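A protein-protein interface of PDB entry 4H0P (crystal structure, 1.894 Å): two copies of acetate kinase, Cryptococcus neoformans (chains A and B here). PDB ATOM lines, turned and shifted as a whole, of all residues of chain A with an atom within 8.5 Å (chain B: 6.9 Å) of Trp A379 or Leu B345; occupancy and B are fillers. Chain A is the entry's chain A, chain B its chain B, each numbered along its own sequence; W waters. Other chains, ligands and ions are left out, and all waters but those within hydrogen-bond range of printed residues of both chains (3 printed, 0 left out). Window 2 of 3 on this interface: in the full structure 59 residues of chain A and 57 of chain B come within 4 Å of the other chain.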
ATOM      1  N   LEU A 334      10.362  21.487   4.382  1.00  0.00           N
ATOM      2  CA  LEU A 334       9.237  21.692   3.462  1.00  0.00           C
ATOM      3  C   LEU A 334       8.213  20.577   3.539  1.00  0.00           C
ATOM      4  O   LEU A 334       7.029  20.827   3.349  1.00  0.00           O
ATOM      5  CB  LEU A 334       9.710  21.819   2.034  1.00  0.00           C
ATOM      6  CG  LEU A 334      10.370  23.166   1.804  1.00  0.00           C
ATOM      7  CD1 LEU A 334      11.082  23.113   0.471  1.00  0.00           C
ATOM      8  CD2 LEU A 334       9.304  24.273   1.846  1.00  0.00           C
ATOM      9  N   ALA A 338       4.426  21.505   4.298  1.00  0.00           N
ATOM     10  CA  ALA A 338       3.402  20.982   3.381  1.00  0.00           C
ATOM     11  C   ALA A 338       2.303  20.201   4.098  1.00  0.00           C
ATOM     12  O   ALA A 338       1.107  20.486   3.893  1.00  0.00           O
ATOM     13  CB  ALA A 338       4.028  20.147   2.301  1.00  0.00           C
ATOM     14  N   LEU A 341       0.274  22.795   6.396  1.00  0.00           N
ATOM     15  CA  LEU A 341      -0.544  23.700   5.589  1.00  0.00           C
ATOM     16  C   LEU A 341      -1.704  22.956   4.956  1.00  0.00           C
ATOM     17  O   LEU A 341      -2.847  23.413   4.964  1.00  0.00           O
ATOM     18  CB  LEU A 341       0.295  24.392   4.514  1.00  0.00           C
ATOM     19  CG  LEU A 341       1.210  25.518   4.991  1.00  0.00           C
ATOM     20  CD1 LEU A 341       1.960  26.113   3.791  1.00  0.00           C
ATOM     21  CD2 LEU A 341       0.421  26.627   5.716  1.00  0.00           C
ATOM     22  N   PHE A 342      -1.411  21.774   4.435  1.00  0.00           N
ATOM     23  CA  PHE A 342      -2.437  20.961   3.839  1.00  0.00           C
ATOM     24  C   PHE A 342      -3.528  20.638   4.840  1.00  0.00           C
ATOM     25  O   PHE A 342      -4.725  20.700   4.523  1.00  0.00           O
ATOM     26  CB  PHE A 342      -1.817  19.662   3.384  1.00  0.00           C
ATOM     27  CG  PHE A 342      -2.742  18.798   2.658  1.00  0.00           C
ATOM     28  CD1 PHE A 342      -3.531  17.876   3.354  1.00  0.00           C
ATOM     29  CD2 PHE A 342      -2.813  18.870   1.267  1.00  0.00           C
ATOM     30  CE1 PHE A 342      -4.396  17.044   2.699  1.00  0.00           C
ATOM     31  CE2 PHE A 342      -3.677  18.043   0.599  1.00  0.00           C
ATOM     32  CZ  PHE A 342      -4.474  17.120   1.317  1.00  0.00           C
ATOM     33  N   LEU A 345      -5.497  23.785   5.542  1.00  0.00           N
ATOM     34  CA  LEU A 345      -6.213  24.269   4.355  1.00  0.00           C
ATOM     35  C   LEU A 345      -7.355  23.355   3.933  1.00  0.00           C
ATOM     36  O   LEU A 345      -8.236  23.775   3.191  1.00  0.00           O
ATOM     37  CB  LEU A 345      -5.252  24.512   3.175  1.00  0.00           C
ATOM     38  CG  LEU A 345      -4.244  25.654   3.334  1.00  0.00           C
ATOM     39  CD1 LEU A 345      -3.157  25.591   2.264  1.00  0.00           C
ATOM     40  CD2 LEU A 345      -4.911  27.034   3.341  1.00  0.00           C
ATOM     41  N   ILE A 350      -7.085  29.909   3.062  1.00  0.00           N
ATOM     42  CA  ILE A 350      -5.794  30.531   3.388  1.00  0.00           C
ATOM     43  C   ILE A 350      -5.936  31.929   4.019  1.00  0.00           C
ATOM     44  O   ILE A 350      -5.121  32.333   4.871  1.00  0.00           O
ATOM     45  CB  ILE A 350      -4.809  30.486   2.170  1.00  0.00           C
ATOM     46  CG1 ILE A 350      -3.359  30.722   2.607  1.00  0.00           C
ATOM     47  CG2 ILE A 350      -5.221  31.459   1.080  1.00  0.00           C
ATOM     48  CD1 ILE A 350      -2.351  29.876   1.837  1.00  0.00           C
ATOM     49  N   VAL A 373      12.009  28.780   1.903  1.00  0.00           N
ATOM     50  CA  VAL A 373      10.722  28.166   2.214  1.00  0.00           C
ATOM     51  C   VAL A 373       9.614  28.978   1.586  1.00  0.00           C
ATOM     52  O   VAL A 373       8.713  28.437   0.939  1.00  0.00           O
ATOM     53  CB  VAL A 373      10.500  28.061   3.741  1.00  0.00           C
ATOM     54  CG1 VAL A 373       9.085  27.584   4.049  1.00  0.00           C
ATOM     55  CG2 VAL A 373      11.514  27.137   4.375  1.00  0.00           C
ATOM     56  N   LEU A 374       9.667  30.297   1.761  1.00  0.00           N
ATOM     57  CA  LEU A 374       8.565  31.118   1.284  1.00  0.00           C
ATOM     58  C   LEU A 374       8.479  31.139  -0.247  1.00  0.00           C
ATOM     59  O   LEU A 374       7.380  31.171  -0.798  1.00  0.00           O
ATOM     60  CB  LEU A 374       8.670  32.534   1.863  1.00  0.00           C
ATOM     61  CG  LEU A 374       8.260  32.655   3.328  1.00  0.00           C
ATOM     62  CD1 LEU A 374       8.681  34.007   3.917  1.00  0.00           C
ATOM     63  CD2 LEU A 374       6.766  32.454   3.492  1.00  0.00           C
ATOM     64  N   LYS A 375       9.628  31.100  -0.924  1.00  0.00           N
ATOM     65  CA  LYS A 375       9.649  30.975  -2.390  1.00  0.00           C
ATOM     66  C   LYS A 375       8.948  29.699  -2.847  1.00  0.00           C
ATOM     67  O   LYS A 375       8.298  29.671  -3.897  1.00  0.00           O
ATOM     68  CB  LYS A 375      11.097  30.934  -2.920  1.00  0.00           C
ATOM     69  CG  LYS A 375      11.949  32.199  -2.660  1.00  0.00           C
ATOM     70  CD  LYS A 375      11.444  33.414  -3.416  1.00  0.00           C
ATOM     71  CE  LYS A 375      12.192  34.677  -2.962  1.00  0.00           C
ATOM     72  NZ  LYS A 375      11.855  35.866  -3.791  1.00  0.00           N
ATOM     73  N   LYS A 376       9.102  28.633  -2.072  1.00  0.00           N
ATOM     74  CA  LYS A 376       8.514  27.349  -2.437  1.00  0.00           C
ATOM     75  C   LYS A 376       7.005  27.403  -2.313  1.00  0.00           C
ATOM     76  O   LYS A 376       6.308  26.603  -2.931  1.00  0.00           O
ATOM     77  CB  LYS A 376       9.074  26.226  -1.560  1.00  0.00           C
ATOM     78  CG  LYS A 376      10.488  25.786  -1.927  1.00  0.00           C
ATOM     79  CD  LYS A 376      10.476  25.093  -3.281  1.00  0.00           C
ATOM     80  CE  LYS A 376      11.613  24.095  -3.399  1.00  0.00           C
ATOM     81  NZ  LYS A 376      12.935  24.762  -3.343  1.00  0.00           N
ATOM     82  N   LEU A 377       6.503  28.359  -1.532  1.00  0.00           N
ATOM     83  CA  LEU A 377       5.056  28.509  -1.339  1.00  0.00           C
ATOM     84  C   LEU A 377       4.447  29.597  -2.229  1.00  0.00           C
ATOM     85  O   LEU A 377       3.331  30.073  -1.986  1.00  0.00           O
ATOM     86  CB  LEU A 377       4.744  28.776   0.133  1.00  0.00           C
ATOM     87  CG  LEU A 377       5.216  27.678   1.080  1.00  0.00           C
ATOM     88  CD1 LEU A 377       5.111  28.159   2.508  1.00  0.00           C
ATOM     89  CD2 LEU A 377       4.389  26.424   0.892  1.00  0.00           C
ATOM     90  N   ALA A 378       5.189  29.977  -3.264  1.00  0.00           N
ATOM     91  CA  ALA A 378       4.750  31.004  -4.198  1.00  0.00           C
ATOM     92  C   ALA A 378       3.462  30.591  -4.882  1.00  0.00           C
ATOM     93  O   ALA A 378       2.631  31.435  -5.179  1.00  0.00           O
ATOM     94  CB  ALA A 378       5.857  31.284  -5.243  1.00  0.00           C
ATOM     95  N   TRP A 379       3.286  29.293  -5.129  1.00  0.00           N
ATOM     96  CA  TRP A 379       2.066  28.805  -5.777  1.00  0.00           C
ATOM     97  C   TRP A 379       0.823  29.010  -4.913  1.00  0.00           C
ATOM     98  O   TRP A 379      -0.289  29.021  -5.425  1.00  0.00           O
ATOM     99  CB  TRP A 379       2.213  27.341  -6.195  1.00  0.00           C
ATOM    100  CG  TRP A 379       2.243  26.385  -5.027  1.00  0.00           C
ATOM    101  CD1 TRP A 379       3.334  26.012  -4.292  1.00  0.00           C
ATOM    102  CD2 TRP A 379       1.130  25.666  -4.489  1.00  0.00           C
ATOM    103  NE1 TRP A 379       2.961  25.115  -3.311  1.00  0.00           N
ATOM    104  CE2 TRP A 379       1.616  24.885  -3.414  1.00  0.00           C
ATOM    105  CE3 TRP A 379      -0.229  25.602  -4.814  1.00  0.00           C
ATOM    106  CZ2 TRP A 379       0.784  24.053  -2.664  1.00  0.00           C
ATOM    107  CZ3 TRP A 379      -1.057  24.786  -4.056  1.00  0.00           C
ATOM    108  CH2 TRP A 379      -0.552  24.023  -3.000  1.00  0.00           C
ATOM    109  N   LEU A 380       1.017  29.181  -3.608  1.00  0.00           N
ATOM    110  CA  LEU A 380      -0.086  29.427  -2.681  1.00  0.00           C
ATOM    111  C   LEU A 380      -0.321  30.927  -2.518  1.00  0.00           C
ATOM    112  O   LEU A 380      -1.293  31.343  -1.885  1.00  0.00           O
ATOM    113  CB  LEU A 380       0.234  28.850  -1.302  1.00  0.00           C
ATOM    114  CG  LEU A 380      -0.003  27.377  -1.024  1.00  0.00           C
ATOM    115  CD1 LEU A 380       0.368  27.057   0.421  1.00  0.00           C
ATOM    116  CD2 LEU A 380      -1.451  27.064  -1.273  1.00  0.00           C
ATOM    117  N   GLY A 381       0.583  31.736  -3.067  1.00  0.00           N
ATOM    118  CA  GLY A 381       0.472  33.184  -2.958  1.00  0.00           C
ATOM    119  C   GLY A 381       1.354  33.851  -1.915  1.00  0.00           C
ATOM    120  O   GLY A 381       1.207  35.041  -1.654  1.00  0.00           O
ATOM    121  N   ALA A 382       2.271  33.108  -1.306  1.00  0.00           N
ATOM    122  CA  ALA A 382       3.205  33.735  -0.381  1.00  0.00           C
ATOM    123  C   ALA A 382       4.197  34.595  -1.164  1.00  0.00           C
ATOM    124  O   ALA A 382       4.672  34.207  -2.226  1.00  0.00           O
ATOM    125  CB  ALA A 382       3.944  32.704   0.459  1.00  0.00           C
ATOM    126  N   GLU A 383       4.510  35.765  -0.629  1.00  0.00           N
ATOM    127  CA  GLU A 383       5.498  36.646  -1.240  1.00  0.00           C
ATOM    128  C   GLU A 383       6.347  37.209  -0.115  1.00  0.00           C
ATOM    129  O   GLU A 383       5.832  37.922   0.765  1.00  0.00           O
ATOM    130  CB  GLU A 383       4.801  37.790  -1.985  1.00  0.00           C
ATOM    131  CG  GLU A 383       3.411  37.447  -2.530  1.00  0.00           C
ATOM    132  CD  GLU A 383       2.621  38.673  -2.978  1.00  0.00           C
ATOM    133  OE1 GLU A 383       3.250  39.675  -3.375  1.00  0.00           O
ATOM    134  OE2 GLU A 383       1.372  38.629  -2.934  1.00  0.00           O
ATOM    135  N   LYS A 406      -0.861  36.235   0.088  1.00  0.00           N
ATOM    136  CA  LYS A 406      -2.029  35.486   0.510  1.00  0.00           C
ATOM    137  C   LYS A 406      -1.719  34.560   1.698  1.00  0.00           C
ATOM    138  O   LYS A 406      -2.615  34.128   2.417  1.00  0.00           O
ATOM    139  CB  LYS A 406      -2.675  34.773  -0.674  1.00  0.00           C
ATOM    140  CG  LYS A 406      -3.284  35.787  -1.651  1.00  0.00           C
ATOM    141  CD  LYS A 406      -3.985  35.120  -2.804  1.00  0.00           C
ATOM    142  CE  LYS A 406      -3.035  34.204  -3.533  1.00  0.00           C
ATOM    143  NZ  LYS A 406      -3.768  33.375  -4.527  1.00  0.00           N
ATOM    144  N   LEU A 407      -0.440  34.301   1.923  1.00  0.00           N
ATOM    145  CA  LEU A 407      -0.003  33.606   3.137  1.00  0.00           C
ATOM    146  C   LEU A 407       0.889  34.536   3.943  1.00  0.00           C
ATOM    147  O   LEU A 407       1.925  34.977   3.434  1.00  0.00           O
ATOM    148  CB  LEU A 407       0.792  32.359   2.763  1.00  0.00           C
ATOM    149  CG  LEU A 407       1.277  31.522   3.944  1.00  0.00           C
ATOM    150  CD1 LEU A 407       0.098  30.783   4.534  1.00  0.00           C
ATOM    151  CD2 LEU A 407       2.374  30.562   3.501  1.00  0.00           C
ATOM    152  N   ALA B 338       0.086  15.213   0.501  1.00  0.00           N
ATOM    153  CA  ALA B 338       0.387  16.631   0.721  1.00  0.00           C
ATOM    154  C   ALA B 338       1.823  16.956   0.367  1.00  0.00           C
ATOM    155  O   ALA B 338       2.078  17.900  -0.401  1.00  0.00           O
ATOM    156  CB  ALA B 338       0.091  17.035   2.160  1.00  0.00           C
ATOM    157  N   TYR B 340       3.877  15.506  -1.582  1.00  0.00           N
ATOM    158  CA  TYR B 340       4.231  15.333  -2.991  1.00  0.00           C
ATOM    159  C   TYR B 340       3.485  16.283  -3.936  1.00  0.00           C
ATOM    160  O   TYR B 340       4.044  16.738  -4.939  1.00  0.00           O
ATOM    161  CB  TYR B 340       4.053  13.860  -3.404  1.00  0.00           C
ATOM    162  CG  TYR B 340       4.912  12.929  -2.563  1.00  0.00           C
ATOM    163  CD1 TYR B 340       6.056  13.409  -1.919  1.00  0.00           C
ATOM    164  CD2 TYR B 340       4.606  11.567  -2.432  1.00  0.00           C
ATOM    165  CE1 TYR B 340       6.848  12.569  -1.144  1.00  0.00           C
ATOM    166  CE2 TYR B 340       5.402  10.727  -1.667  1.00  0.00           C
ATOM    167  CZ  TYR B 340       6.514  11.242  -1.015  1.00  0.00           C
ATOM    168  OH  TYR B 340       7.309  10.424  -0.238  1.00  0.00           O
ATOM    169  N   LEU B 341       2.216  16.550  -3.658  1.00  0.00           N
ATOM    170  CA  LEU B 341       1.512  17.595  -4.414  1.00  0.00           C
ATOM    171  C   LEU B 341       2.222  18.933  -4.215  1.00  0.00           C
ATOM    172  O   LEU B 341       2.447  19.664  -5.173  1.00  0.00           O
ATOM    173  CB  LEU B 341       0.042  17.712  -4.008  1.00  0.00           C
ATOM    174  CG  LEU B 341      -0.871  16.628  -4.566  1.00  0.00           C
ATOM    175  CD1 LEU B 341      -2.291  16.824  -4.026  1.00  0.00           C
ATOM    176  CD2 LEU B 341      -0.868  16.652  -6.100  1.00  0.00           C
ATOM    177  N   PHE B 342       2.620  19.241  -2.983  1.00  0.00           N
ATOM    178  CA  PHE B 342       3.300  20.508  -2.742  1.00  0.00           C
ATOM    179  C   PHE B 342       4.597  20.539  -3.511  1.00  0.00           C
ATOM    180  O   PHE B 342       4.939  21.549  -4.148  1.00  0.00           O
ATOM    181  CB  PHE B 342       3.585  20.701  -1.244  1.00  0.00           C
ATOM    182  CG  PHE B 342       2.523  21.491  -0.510  1.00  0.00           C
ATOM    183  CD1 PHE B 342       1.241  20.953  -0.306  1.00  0.00           C
ATOM    184  CD2 PHE B 342       2.821  22.752   0.014  1.00  0.00           C
ATOM    185  CE1 PHE B 342       0.258  21.657   0.385  1.00  0.00           C
ATOM    186  CE2 PHE B 342       1.846  23.487   0.721  1.00  0.00           C
ATOM    187  CZ  PHE B 342       0.564  22.934   0.911  1.00  0.00           C
ATOM    188  N   LYS B 343       5.316  19.421  -3.483  1.00  0.00           N
ATOM    189  CA  LYS B 343       6.569  19.309  -4.219  1.00  0.00           C
ATOM    190  C   LYS B 343       6.390  19.583  -5.726  1.00  0.00           C
ATOM    191  O   LYS B 343       7.147  20.373  -6.328  1.00  0.00           O
ATOM    192  CB  LYS B 343       7.184  17.933  -3.971  1.00  0.00           C
ATOM    193  CG  LYS B 343       8.684  17.905  -4.033  1.00  0.00           C
ATOM    194  CD  LYS B 343       9.201  16.476  -3.892  1.00  0.00           C
ATOM    195  CE  LYS B 343      10.698  16.474  -3.662  1.00  0.00           C
ATOM    196  NZ  LYS B 343      10.986  16.752  -2.214  1.00  0.00           N
ATOM    197  N   LEU B 344       5.382  18.969  -6.345  1.00  0.00           N
ATOM    198  CA  LEU B 344       5.082  19.273  -7.750  1.00  0.00           C
ATOM    199  C   LEU B 344       4.602  20.709  -7.947  1.00  0.00           C
ATOM    200  O   LEU B 344       5.101  21.440  -8.818  1.00  0.00           O
ATOM    201  CB  LEU B 344       4.018  18.313  -8.300  1.00  0.00           C
ATOM    202  CG  LEU B 344       4.462  16.917  -8.646  1.00  0.00           C
ATOM    203  CD1 LEU B 344       3.289  16.112  -9.267  1.00  0.00           C
ATOM    204  CD2 LEU B 344       5.638  17.003  -9.619  1.00  0.00           C
ATOM    205  N   LEU B 345       3.632  21.125  -7.138  1.00  0.00           N
ATOM    206  CA  LEU B 345       3.019  22.441  -7.319  1.00  0.00           C
ATOM    207  C   LEU B 345       4.000  23.574  -7.078  1.00  0.00           C
ATOM    208  O   LEU B 345       3.765  24.699  -7.511  1.00  0.00           O
ATOM    209  CB  LEU B 345       1.794  22.609  -6.415  1.00  0.00           C
ATOM    210  CG  LEU B 345       0.675  21.654  -6.792  1.00  0.00           C
ATOM    211  CD1 LEU B 345      -0.362  21.602  -5.658  1.00  0.00           C
ATOM    212  CD2 LEU B 345       0.033  22.074  -8.100  1.00  0.00           C
ATOM    213  N   SER B 346       5.106  23.281  -6.401  1.00  0.00           N
ATOM    214  CA  SER B 346       6.109  24.304  -6.121  1.00  0.00           C
ATOM    215  C   SER B 346       6.815  24.729  -7.414  1.00  0.00           C
ATOM    216  O   SER B 346       7.484  25.767  -7.468  1.00  0.00           O
ATOM    217  CB  SER B 346       7.127  23.794  -5.102  1.00  0.00           C
ATOM    218  OG  SER B 346       8.086  22.955  -5.705  1.00  0.00           O
ATOM    219  N   GLU B 347       6.666  23.924  -8.460  1.00  0.00           N
ATOM    220  CA  GLU B 347       7.293  24.251  -9.744  1.00  0.00           C
ATOM    221  C   GLU B 347       6.341  24.357 -10.938  1.00  0.00           C
ATOM    222  O   GLU B 347       6.582  25.136 -11.865  1.00  0.00           O
ATOM    223  CB  GLU B 347       8.439  23.281 -10.040  1.00  0.00           C
ATOM    224  CG  GLU B 347       9.596  23.430  -9.049  1.00  0.00           C
ATOM    225  CD  GLU B 347      10.831  22.630  -9.437  1.00  0.00           C
ATOM    226  OE1 GLU B 347      11.204  22.632 -10.635  1.00  0.00           O
ATOM    227  OE2 GLU B 347      11.428  22.004  -8.530  1.00  0.00           O
ATOM    228  N   VAL B 348       5.266  23.583 -10.933  1.00  0.00           N
ATOM    229  CA  VAL B 348       4.367  23.603 -12.085  1.00  0.00           C
ATOM    230  C   VAL B 348       2.953  23.957 -11.659  1.00  0.00           C
ATOM    231  O   VAL B 348       2.519  23.603 -10.555  1.00  0.00           O
ATOM    232  CB  VAL B 348       4.398  22.280 -12.869  1.00  0.00           C
ATOM    233  CG1 VAL B 348       5.760  22.071 -13.505  1.00  0.00           C
ATOM    234  CG2 VAL B 348       4.078  21.133 -11.961  1.00  0.00           C
ATOM    235  N   PRO B 349       2.233  24.690 -12.521  1.00  0.00           N
ATOM    236  CA  PRO B 349       0.842  25.040 -12.211  1.00  0.00           C
ATOM    237  C   PRO B 349      -0.006  23.777 -12.092  1.00  0.00           C
ATOM    238  O   PRO B 349       0.324  22.769 -12.727  1.00  0.00           O
ATOM    239  CB  PRO B 349       0.410  25.852 -13.436  1.00  0.00           C
ATOM    240  CG  PRO B 349       1.350  25.419 -14.538  1.00  0.00           C
ATOM    241  CD  PRO B 349       2.655  25.186 -13.844  1.00  0.00           C
ATOM    242  N   ILE B 350      -1.073  23.809 -11.301  1.00  0.00           N
ATOM    243  CA  ILE B 350      -1.875  22.605 -11.110  1.00  0.00           C
ATOM    244  C   ILE B 350      -2.500  22.124 -12.421  1.00  0.00           C
ATOM    245  O   ILE B 350      -2.763  20.929 -12.600  1.00  0.00           O
ATOM    246  CB  ILE B 350      -2.945  22.788 -10.004  1.00  0.00           C
ATOM    247  CG1 ILE B 350      -3.525  21.436  -9.585  1.00  0.00           C
ATOM    248  CG2 ILE B 350      -4.041  23.749 -10.450  1.00  0.00           C
ATOM    249  CD1 ILE B 350      -4.299  21.484  -8.275  1.00  0.00           C
ATOM    250  N   GLU B 351      -2.691  23.059 -13.347  1.00  0.00           N
ATOM    251  CA  GLU B 351      -3.307  22.772 -14.637  1.00  0.00           C
ATOM    252  C   GLU B 351      -2.460  21.842 -15.484  1.00  0.00           C
ATOM    253  O   GLU B 351      -2.973  21.167 -16.374  1.00  0.00           O
ATOM    254  CB  GLU B 351      -3.568  24.075 -15.406  1.00  0.00           C
ATOM    255  CG  GLU B 351      -4.592  25.009 -14.739  1.00  0.00           C
ATOM    256  CD  GLU B 351      -4.059  25.723 -13.490  1.00  0.00           C
ATOM    257  OE1 GLU B 351      -4.885  26.072 -12.621  1.00  0.00           O
ATOM    258  OE2 GLU B 351      -2.828  25.942 -13.379  1.00  0.00           O
ATOM    259  N   ILE B 353      -0.377  19.458 -14.111  1.00  0.00           N
ATOM    260  CA  ILE B 353      -0.089  18.133 -13.560  1.00  0.00           C
ATOM    261  C   ILE B 353      -1.172  17.153 -13.981  1.00  0.00           C
ATOM    262  O   ILE B 353      -2.332  17.515 -14.136  1.00  0.00           O
ATOM    263  CB  ILE B 353       0.204  18.107 -12.041  1.00  0.00           C
ATOM    264  CG1 ILE B 353      -1.050  18.289 -11.205  1.00  0.00           C
ATOM    265  CG2 ILE B 353       1.206  19.157 -11.678  1.00  0.00           C
ATOM    266  CD1 ILE B 353      -0.787  18.005  -9.722  1.00  0.00           C
ATOM    267  N   TRP B 379     -10.072  21.937  -1.313  1.00  0.00           N
ATOM    268  CA  TRP B 379      -9.470  23.269  -1.335  1.00  0.00           C
ATOM    269  C   TRP B 379      -8.582  23.499  -2.570  1.00  0.00           C
ATOM    270  O   TRP B 379      -8.346  24.633  -2.965  1.00  0.00           O
ATOM    271  CB  TRP B 379      -8.685  23.522  -0.040  1.00  0.00           C
ATOM    272  CG  TRP B 379      -7.399  22.731   0.056  1.00  0.00           C
ATOM    273  CD1 TRP B 379      -7.269  21.444   0.481  1.00  0.00           C
ATOM    274  CD2 TRP B 379      -6.075  23.183  -0.252  1.00  0.00           C
ATOM    275  NE1 TRP B 379      -5.951  21.067   0.455  1.00  0.00           N
ATOM    276  CE2 TRP B 379      -5.197  22.111   0.000  1.00  0.00           C
ATOM    277  CE3 TRP B 379      -5.547  24.386  -0.724  1.00  0.00           C
ATOM    278  CZ2 TRP B 379      -3.817  22.204  -0.202  1.00  0.00           C
ATOM    279  CZ3 TRP B 379      -4.184  24.478  -0.928  1.00  0.00           C
ATOM    280  CH2 TRP B 379      -3.331  23.396  -0.663  1.00  0.00           C
ATOM    281  N   LEU B 380      -8.084  22.424  -3.172  1.00  0.00           N
ATOM    282  CA  LEU B 380      -7.297  22.544  -4.396  1.00  0.00           C
ATOM    283  C   LEU B 380      -8.179  22.497  -5.630  1.00  0.00           C
ATOM    284  O   LEU B 380      -7.699  22.713  -6.748  1.00  0.00           O
ATOM    285  CB  LEU B 380      -6.257  21.430  -4.501  1.00  0.00           C
ATOM    286  CG  LEU B 380      -4.991  21.510  -3.664  1.00  0.00           C
ATOM    287  CD1 LEU B 380      -4.192  20.232  -3.883  1.00  0.00           C
ATOM    288  CD2 LEU B 380      -4.161  22.746  -4.025  1.00  0.00           C
ATOM    289  N   LEU B 407      -8.039  19.328 -10.112  1.00  0.00           N
ATOM    290  CA  LEU B 407      -7.061  18.260  -9.897  1.00  0.00           C
ATOM    291  C   LEU B 407      -7.656  16.964 -10.428  1.00  0.00           C
ATOM    292  O   LEU B 407      -8.704  16.529  -9.962  1.00  0.00           O
ATOM    293  CB  LEU B 407      -6.723  18.121  -8.405  1.00  0.00           C
ATOM    294  CG  LEU B 407      -5.774  16.969  -8.049  1.00  0.00           C
ATOM    295  CD1 LEU B 407      -4.434  17.185  -8.708  1.00  0.00           C
ATOM    296  CD2 LEU B 407      -5.618  16.814  -6.532  1.00  0.00           C
HETATM  297  O   HOH W   1       5.059  23.863  -2.174  1.00  0.00           O
HETATM  298  O   HOH W   2       5.671  27.928  -5.744  1.00  0.00           O
HETATM  299  O   HOH W   3      -6.122  19.315   2.330  1.00  0.00           O
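The backbone carbonyl oxygen (O) of Leu A377 is in hydrogen-bond range of the backbone NH (N) of Ala A382. The backbone carbonyl oxygen (O) of Lys B343 sits at hydrogen-bond distance from the side-chain hydroxyl (OG) of Ser B346, at 2.8 Å.
Among the printed residues, merely in contact across the chains: Ala A338 with Ala B338 (3.99 Å), Ala A338 with Phe B342 (3.5 Å), Leu A341 with Phe B342 (3.9 Å), Phe A342 with Ala B338 (3.4 Å), Phe A342 with Trp B379 (3.8 Å), Leu A345 with Trp B379 (3.3 Å), Lys A376 with Ser B346 (3.6 Å), Leu A377 with Phe B342 (3.9 Å), Trp A379 with Phe B342 (3.6 Å), Trp A379 with Leu B345 (3.3 Å), Trp A379 with Ser B346 (3.7 Å), Trp A379 with Trp B379 (3.7 Å), Trp A379 with Leu B380 (3.7 Å), Leu A380 with Phe B342 (3.9 Å) and Leu A380 with Trp B379 (3.8 Å).
Printed residues of chain B within 4 Å of Ala A338: Ala B338 and Phe B342. Of the printed residues of chain B, Leu A341 touches Phe B342 (3.9 Å). Printed residues of chain B within 4 Å of Leu A345: Trp B379. Of chain B, only Phe B342, Leu B345, Ser B346, Trp B379 and Leu B380 come within 4 Å of Trp A379. Leu B345 touches just one residue of chain A: Trp A379. Of chain A, only Lys A376 (3.6 Å) and Trp A379 (3.7 Å) come within 4 Å of Ser B346. Printed residues of chain A within 4 Å of Leu B380: Trp A379 (3.7 Å). The nearest residue of chain B that does not touch Trp A379 is Leu B341 (5.3 Å). The nearest residue of chain A that does not touch Leu B345 is Lys A376 (5.6 Å). The nearest printed residue of chain B that does not touch Leu A380 is Leu B380 (5.8 Å).
Hydrophobic or aromatic side chains of chain A within 4 Å of the printed part of chain B: Ala A338, Leu A341, Phe A342, Leu A345, Leu A377, Trp A379 and Leu A380. Along chain A the printed residues that touch a printed residue of chain B span positions 338 to 380. Among the printed residues, no Asp or Glu carboxylate lies within 4 Å of a Lys or Arg side-chain nitrogen of the other chain.
Ala A338 touches Phe B342, and with the chains exchanged Phe A342 touches Ala B338. Leu A341 touches Phe B342, but with the chains exchanged Phe A342 does not touch Leu B341 (5.0 Å). Phe A342 touches Trp B379, and with the chains exchanged Trp A379 touches Phe B342. Leu A380 touches Phe B342, but with the chains exchanged Phe A342 does not touch Leu B380 (5.0 Å). Of the 15 pairs that touch across the chains among the printed residues, 10 have their exchanged pair printed and touching as well.
Water W3 lies within hydrogen-bond range of NE1 of Trp B379 (2.6 Å) and O of Phe A342 (2.9 Å). Water W1 lies within hydrogen-bond range of NE1 of Trp A379 (2.7 Å), O of Phe B342 (3.0 Å) and O of Lys A376 (3.1 Å). Water W2 lies within hydrogen-bond range of N of Trp A379 (2.8 Å), O of Lys A376 (3.2 Å), N of Ala A378 (3.3 Å) and O of Ser B346 (3.3 Å).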
